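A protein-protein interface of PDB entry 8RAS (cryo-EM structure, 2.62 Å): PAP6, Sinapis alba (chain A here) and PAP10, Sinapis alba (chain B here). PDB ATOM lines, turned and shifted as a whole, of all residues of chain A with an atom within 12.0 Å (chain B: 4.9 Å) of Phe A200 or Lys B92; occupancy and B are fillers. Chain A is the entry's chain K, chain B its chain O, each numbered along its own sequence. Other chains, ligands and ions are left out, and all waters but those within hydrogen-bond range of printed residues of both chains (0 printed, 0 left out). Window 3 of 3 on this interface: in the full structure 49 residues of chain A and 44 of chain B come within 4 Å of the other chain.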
ATOM      1  N   VAL A 196     -19.995 -25.328  -7.459  1.00  0.00           N
ATOM      2  CA  VAL A 196     -18.977 -25.879  -8.339  1.00  0.00           C
ATOM      3  C   VAL A 196     -17.615 -25.716  -7.681  1.00  0.00           C
ATOM      4  O   VAL A 196     -17.406 -24.848  -6.832  1.00  0.00           O
ATOM      5  CB  VAL A 196     -18.981 -25.213  -9.733  1.00  0.00           C
ATOM      6  CG1 VAL A 196     -20.205 -25.645 -10.526  1.00  0.00           C
ATOM      7  CG2 VAL A 196     -18.929 -23.702  -9.600  1.00  0.00           C
ATOM      8  N   LYS A 197     -16.680 -26.569  -8.092  1.00  0.00           N
ATOM      9  CA  LYS A 197     -15.305 -26.529  -7.615  1.00  0.00           C
ATOM     10  C   LYS A 197     -14.381 -26.262  -8.792  1.00  0.00           C
ATOM     11  O   LYS A 197     -14.444 -26.966  -9.806  1.00  0.00           O
ATOM     12  CB  LYS A 197     -14.918 -27.836  -6.920  1.00  0.00           C
ATOM     13  CG  LYS A 197     -14.969 -27.769  -5.403  1.00  0.00           C
ATOM     14  CD  LYS A 197     -13.885 -28.628  -4.773  1.00  0.00           C
ATOM     15  CE  LYS A 197     -12.804 -27.774  -4.131  1.00  0.00           C
ATOM     16  NZ  LYS A 197     -11.820 -28.594  -3.375  1.00  0.00           N
ATOM     17  N   ILE A 198     -13.526 -25.257  -8.656  1.00  0.00           N
ATOM     18  CA  ILE A 198     -12.650 -24.827  -9.740  1.00  0.00           C
ATOM     19  C   ILE A 198     -11.338 -25.595  -9.647  1.00  0.00           C
ATOM     20  O   ILE A 198     -10.674 -25.588  -8.605  1.00  0.00           O
ATOM     21  CB  ILE A 198     -12.408 -23.312  -9.686  1.00  0.00           C
ATOM     22  CG1 ILE A 198     -13.696 -22.557 -10.014  1.00  0.00           C
ATOM     23  CG2 ILE A 198     -11.306 -22.914 -10.648  1.00  0.00           C
ATOM     24  CD1 ILE A 198     -13.589 -21.065  -9.827  1.00  0.00           C
ATOM     25  N   LYS A 199     -10.964 -26.255 -10.740  1.00  0.00           N
ATOM     26  CA  LYS A 199      -9.733 -27.026 -10.819  1.00  0.00           C
ATOM     27  C   LYS A 199      -8.927 -26.564 -12.025  1.00  0.00           C
ATOM     28  O   LYS A 199      -9.414 -25.825 -12.883  1.00  0.00           O
ATOM     29  CB  LYS A 199     -10.021 -28.532 -10.903  1.00  0.00           C
ATOM     30  CG  LYS A 199     -10.753 -28.953 -12.163  1.00  0.00           C
ATOM     31  CD  LYS A 199     -11.051 -30.443 -12.150  1.00  0.00           C
ATOM     32  CE  LYS A 199     -11.476 -30.934 -13.525  1.00  0.00           C
ATOM     33  NZ  LYS A 199     -12.857 -30.500 -13.868  1.00  0.00           N
ATOM     34  N   PHE A 200      -7.676 -27.013 -12.084  1.00  0.00           N
ATOM     35  CA  PHE A 200      -6.717 -26.581 -13.097  1.00  0.00           C
ATOM     36  C   PHE A 200      -6.105 -27.785 -13.802  1.00  0.00           C
ATOM     37  O   PHE A 200      -4.885 -27.916 -13.926  1.00  0.00           O
ATOM     38  CB  PHE A 200      -5.640 -25.698 -12.475  1.00  0.00           C
ATOM     39  CG  PHE A 200      -6.165 -24.400 -11.940  1.00  0.00           C
ATOM     40  CD1 PHE A 200      -6.629 -24.309 -10.638  1.00  0.00           C
ATOM     41  CD2 PHE A 200      -6.210 -23.273 -12.741  1.00  0.00           C
ATOM     42  CE1 PHE A 200      -7.117 -23.116 -10.143  1.00  0.00           C
ATOM     43  CE2 PHE A 200      -6.698 -22.078 -12.253  1.00  0.00           C
ATOM     44  CZ  PHE A 200      -7.152 -21.999 -10.952  1.00  0.00           C
ATOM     45  N   GLU A 201      -6.963 -28.694 -14.259  1.00  0.00           N
ATOM     46  CA  GLU A 201      -6.504 -29.870 -14.984  1.00  0.00           C
ATOM     47  C   GLU A 201      -5.746 -29.472 -16.246  1.00  0.00           C
ATOM     48  O   GLU A 201      -6.160 -28.570 -16.980  1.00  0.00           O
ATOM     49  CB  GLU A 201      -7.694 -30.760 -15.346  1.00  0.00           C
ATOM     50  CG  GLU A 201      -7.310 -32.100 -15.949  1.00  0.00           C
ATOM     51  CD  GLU A 201      -8.478 -32.782 -16.636  1.00  0.00           C
ATOM     52  OE1 GLU A 201      -9.406 -32.071 -17.076  1.00  0.00           O
ATOM     53  OE2 GLU A 201      -8.470 -34.027 -16.733  1.00  0.00           O
ATOM     54  N   ASP A 202      -4.626 -30.160 -16.486  1.00  0.00           N
ATOM     55  CA  ASP A 202      -3.756 -29.994 -17.650  1.00  0.00           C
ATOM     56  C   ASP A 202      -3.534 -28.536 -18.043  1.00  0.00           C
ATOM     57  O   ASP A 202      -3.493 -28.203 -19.232  1.00  0.00           O
ATOM     58  CB  ASP A 202      -4.298 -30.800 -18.842  1.00  0.00           C
ATOM     59  CG  ASP A 202      -5.618 -30.270 -19.376  1.00  0.00           C
ATOM     60  OD1 ASP A 202      -6.678 -30.645 -18.834  1.00  0.00           O
ATOM     61  OD2 ASP A 202      -5.598 -29.493 -20.353  1.00  0.00           O
ATOM     62  N   GLY A 203      -3.360 -27.663 -17.053  1.00  0.00           N
ATOM     63  CA  GLY A 203      -3.035 -26.278 -17.318  1.00  0.00           C
ATOM     64  C   GLY A 203      -4.185 -25.412 -17.779  1.00  0.00           C
ATOM     65  O   GLY A 203      -3.949 -24.275 -18.203  1.00  0.00           O
ATOM     66  N   LYS A 204      -5.418 -25.907 -17.713  1.00  0.00           N
ATOM     67  CA  LYS A 204      -6.592 -25.139 -18.098  1.00  0.00           C
ATOM     68  C   LYS A 204      -7.595 -25.147 -16.957  1.00  0.00           C
ATOM     69  O   LYS A 204      -7.825 -26.184 -16.328  1.00  0.00           O
ATOM     70  CB  LYS A 204      -7.237 -25.702 -19.369  1.00  0.00           C
ATOM     71  CG  LYS A 204      -6.398 -25.528 -20.624  1.00  0.00           C
ATOM     72  CD  LYS A 204      -7.121 -26.056 -21.853  1.00  0.00           C
ATOM     73  CE  LYS A 204      -7.747 -27.416 -21.588  1.00  0.00           C
ATOM     74  NZ  LYS A 204      -8.693 -27.816 -22.666  1.00  0.00           N
ATOM     75  N   MET A 205      -8.189 -23.986 -16.692  1.00  0.00           N
ATOM     76  CA  MET A 205      -9.176 -23.880 -15.627  1.00  0.00           C
ATOM     77  C   MET A 205     -10.447 -24.631 -16.002  1.00  0.00           C
ATOM     78  O   MET A 205     -10.935 -24.537 -17.131  1.00  0.00           O
ATOM     79  CB  MET A 205      -9.498 -22.415 -15.345  1.00  0.00           C
ATOM     80  CG  MET A 205     -10.102 -22.161 -13.980  1.00  0.00           C
ATOM     81  SD  MET A 205      -9.834 -20.473 -13.410  1.00  0.00           S
ATOM     82  CE  MET A 205     -11.283 -19.659 -14.071  1.00  0.00           C
ATOM     83  N   LYS A 206     -10.983 -25.379 -15.041  1.00  0.00           N
ATOM     84  CA  LYS A 206     -12.193 -26.160 -15.250  1.00  0.00           C
ATOM     85  C   LYS A 206     -13.003 -26.160 -13.964  1.00  0.00           C
ATOM     86  O   LYS A 206     -12.492 -25.846 -12.886  1.00  0.00           O
ATOM     87  CB  LYS A 206     -11.878 -27.597 -15.681  1.00  0.00           C
ATOM     88  CG  LYS A 206     -11.318 -27.721 -17.086  1.00  0.00           C
ATOM     89  CD  LYS A 206     -10.788 -29.118 -17.347  1.00  0.00           C
ATOM     90  CE  LYS A 206      -9.848 -29.135 -18.539  1.00  0.00           C
ATOM     91  NZ  LYS A 206     -10.533 -28.730 -19.796  1.00  0.00           N
ATOM     92  N   ALA A 207     -14.276 -26.515 -14.090  1.00  0.00           N
ATOM     93  CA  ALA A 207     -15.181 -26.581 -12.955  1.00  0.00           C
ATOM     94  C   ALA A 207     -15.921 -27.909 -12.964  1.00  0.00           C
ATOM     95  O   ALA A 207     -16.140 -28.510 -14.018  1.00  0.00           O
ATOM     96  CB  ALA A 207     -16.187 -25.423 -12.968  1.00  0.00           C
ATOM     97  N   GLU A 208     -16.290 -28.370 -11.772  1.00  0.00           N
ATOM     98  CA  GLU A 208     -17.087 -29.577 -11.618  1.00  0.00           C
ATOM     99  C   GLU A 208     -18.171 -29.323 -10.585  1.00  0.00           C
ATOM    100  O   GLU A 208     -17.937 -28.643  -9.582  1.00  0.00           O
ATOM    101  CB  GLU A 208     -16.226 -30.778 -11.206  1.00  0.00           C
ATOM    102  CG  GLU A 208     -15.216 -30.483 -10.114  1.00  0.00           C
ATOM    103  CD  GLU A 208     -14.427 -31.712  -9.712  1.00  0.00           C
ATOM    104  OE1 GLU A 208     -15.012 -32.816  -9.700  1.00  0.00           O
ATOM    105  OE2 GLU A 208     -13.223 -31.577  -9.410  1.00  0.00           O
ATOM    106  N   LEU B  87      -8.169 -14.593 -16.719  1.00  0.00           N
ATOM    107  CA  LEU B  87      -9.035 -15.064 -15.643  1.00  0.00           C
ATOM    108  C   LEU B  87      -8.381 -16.201 -14.870  1.00  0.00           C
ATOM    109  O   LEU B  87      -8.540 -16.301 -13.648  1.00  0.00           O
ATOM    110  CB  LEU B  87     -10.385 -15.499 -16.209  1.00  0.00           C
ATOM    111  CG  LEU B  87     -11.475 -15.791 -15.179  1.00  0.00           C
ATOM    112  CD1 LEU B  87     -11.846 -14.531 -14.421  1.00  0.00           C
ATOM    113  CD2 LEU B  87     -12.691 -16.389 -15.854  1.00  0.00           C
ATOM    114  N   GLN B  88      -7.647 -17.070 -15.568  1.00  0.00           N
ATOM    115  CA  GLN B  88      -6.912 -18.138 -14.897  1.00  0.00           C
ATOM    116  C   GLN B  88      -5.891 -17.564 -13.926  1.00  0.00           C
ATOM    117  O   GLN B  88      -5.771 -18.023 -12.784  1.00  0.00           O
ATOM    118  CB  GLN B  88      -6.220 -19.020 -15.934  1.00  0.00           C
ATOM    119  CG  GLN B  88      -7.047 -20.189 -16.413  1.00  0.00           C
ATOM    120  CD  GLN B  88      -6.271 -21.111 -17.330  1.00  0.00           C
ATOM    121  OE1 GLN B  88      -5.380 -21.837 -16.890  1.00  0.00           O
ATOM    122  NE2 GLN B  88      -6.604 -21.085 -18.614  1.00  0.00           N
ATOM    123  N   ASP B  89      -5.144 -16.553 -14.370  1.00  0.00           N
ATOM    124  CA  ASP B  89      -4.161 -15.917 -13.497  1.00  0.00           C
ATOM    125  C   ASP B  89      -4.837 -15.219 -12.324  1.00  0.00           C
ATOM    126  O   ASP B  89      -4.328 -15.247 -11.198  1.00  0.00           O
ATOM    127  CB  ASP B  89      -3.313 -14.929 -14.296  1.00  0.00           C
ATOM    128  CG  ASP B  89      -2.345 -15.621 -15.231  1.00  0.00           C
ATOM    129  OD1 ASP B  89      -1.488 -16.387 -14.742  1.00  0.00           O
ATOM    130  OD2 ASP B  89      -2.440 -15.400 -16.456  1.00  0.00           O
ATOM    131  N   LEU B  90      -5.980 -14.576 -12.572  1.00  0.00           N
ATOM    132  CA  LEU B  90      -6.702 -13.900 -11.500  1.00  0.00           C
ATOM    133  C   LEU B  90      -7.181 -14.887 -10.443  1.00  0.00           C
ATOM    134  O   LEU B  90      -7.074 -14.622  -9.241  1.00  0.00           O
ATOM    135  CB  LEU B  90      -7.883 -13.120 -12.077  1.00  0.00           C
ATOM    136  CG  LEU B  90      -8.270 -11.820 -11.374  1.00  0.00           C
ATOM    137  CD1 LEU B  90      -7.157 -10.795 -11.497  1.00  0.00           C
ATOM    138  CD2 LEU B  90      -9.566 -11.278 -11.947  1.00  0.00           C
ATOM    139  N   VAL B  91      -7.717 -16.031 -10.873  1.00  0.00           N
ATOM    140  CA  VAL B  91      -8.205 -17.023  -9.921  1.00  0.00           C
ATOM    141  C   VAL B  91      -7.044 -17.674  -9.181  1.00  0.00           C
ATOM    142  O   VAL B  91      -7.123 -17.924  -7.972  1.00  0.00           O
ATOM    143  CB  VAL B  91      -9.080 -18.065 -10.641  1.00  0.00           C
ATOM    144  CG1 VAL B  91      -9.450 -19.197  -9.699  1.00  0.00           C
ATOM    145  CG2 VAL B  91     -10.331 -17.405 -11.192  1.00  0.00           C
ATOM    146  N   LYS B  92      -5.945 -17.951  -9.887  1.00  0.00           N
ATOM    147  CA  LYS B  92      -4.781 -18.551  -9.244  1.00  0.00           C
ATOM    148  C   LYS B  92      -4.171 -17.613  -8.210  1.00  0.00           C
ATOM    149  O   LYS B  92      -3.744 -18.053  -7.136  1.00  0.00           O
ATOM    150  CB  LYS B  92      -3.739 -18.933 -10.294  1.00  0.00           C
ATOM    151  CG  LYS B  92      -3.982 -20.277 -10.949  1.00  0.00           C
ATOM    152  CD  LYS B  92      -2.745 -20.763 -11.683  1.00  0.00           C
ATOM    153  CE  LYS B  92      -3.052 -21.066 -13.138  1.00  0.00           C
ATOM    154  NZ  LYS B  92      -2.068 -20.430 -14.056  1.00  0.00           N
ATOM    155  N   GLY B  93      -4.122 -16.321  -8.512  1.00  0.00           N
ATOM    156  CA  GLY B  93      -3.501 -15.367  -7.618  1.00  0.00           C
ATOM    157  C   GLY B  93      -4.307 -15.133  -6.356  1.00  0.00           C
ATOM    158  O   GLY B  93      -5.483 -15.484  -6.242  1.00  0.00           O
ATOM    159  N   GLU B  94      -3.642 -14.523  -5.378  1.00  0.00           N
ATOM    160  CA  GLU B  94      -4.285 -14.208  -4.111  1.00  0.00           C
ATOM    161  C   GLU B  94      -5.387 -13.176  -4.316  1.00  0.00           C
ATOM    162  O   GLU B  94      -5.212 -12.191  -5.039  1.00  0.00           O
ATOM    163  CB  GLU B  94      -3.252 -13.690  -3.109  1.00  0.00           C
ATOM    164  CG  GLU B  94      -3.845 -13.081  -1.848  1.00  0.00           C
ATOM    165  CD  GLU B  94      -4.294 -14.131  -0.849  1.00  0.00           C
ATOM    166  OE1 GLU B  94      -3.589 -15.150  -0.699  1.00  0.00           O
ATOM    167  OE2 GLU B  94      -5.352 -13.935  -0.215  1.00  0.00           O
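Phe A200 touches two residues of chain B.
Lys B92 touches just one residue of chain A: Phe A200 (3.5 Å).
Of chain A, only Gly A203 (3.1 Å), Lys A204 (3.7 Å) and Met A205 (3.5 Å) come within 4 Å of Gln B88.
No residue of chain A comes within 4 Å of Asp B89.
Leu B90 touches none of the printed residues of chain A.
No residue of chain A comes within 4 Å of Gly B93.
Of the printed residues of chain B, Gly A203 touches Gln B88 (3.1 Å).
Of the printed residues of chain A, Leu B87 touches Met A205.
Glu A201 touches none of the printed residues of chain B.
The nearest residue of chain B that does not touch Phe A200 is Gln B88 (4.2 Å).
The nearest residue of chain A that does not touch Lys B92 is Met A205 (5.8 Å).
The nearest printed residue of chain A that does not touch Leu B87 is Phe A200 (6.2 Å).
Of the 13 printed residues of chain A, 4 touch a printed residue of chain B.
Hydrophobic or aromatic side chains of chain A within 4 Å of the printed part of chain B: Phe A200 and Met A205.
Among the printed residues, 7 pairs touch across the chains.
Among the printed residues, merely in contact across the chains: Met A205 with Gln B88, Phe A200 with Lys B92, Lys A204 with Gln B88, Met A205 with Val B91, Phe A200 with Val B91 and Met A205 with Leu B87.
O of Gly A203 lies close to OE1 of Gln B88 (3.1 Å).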
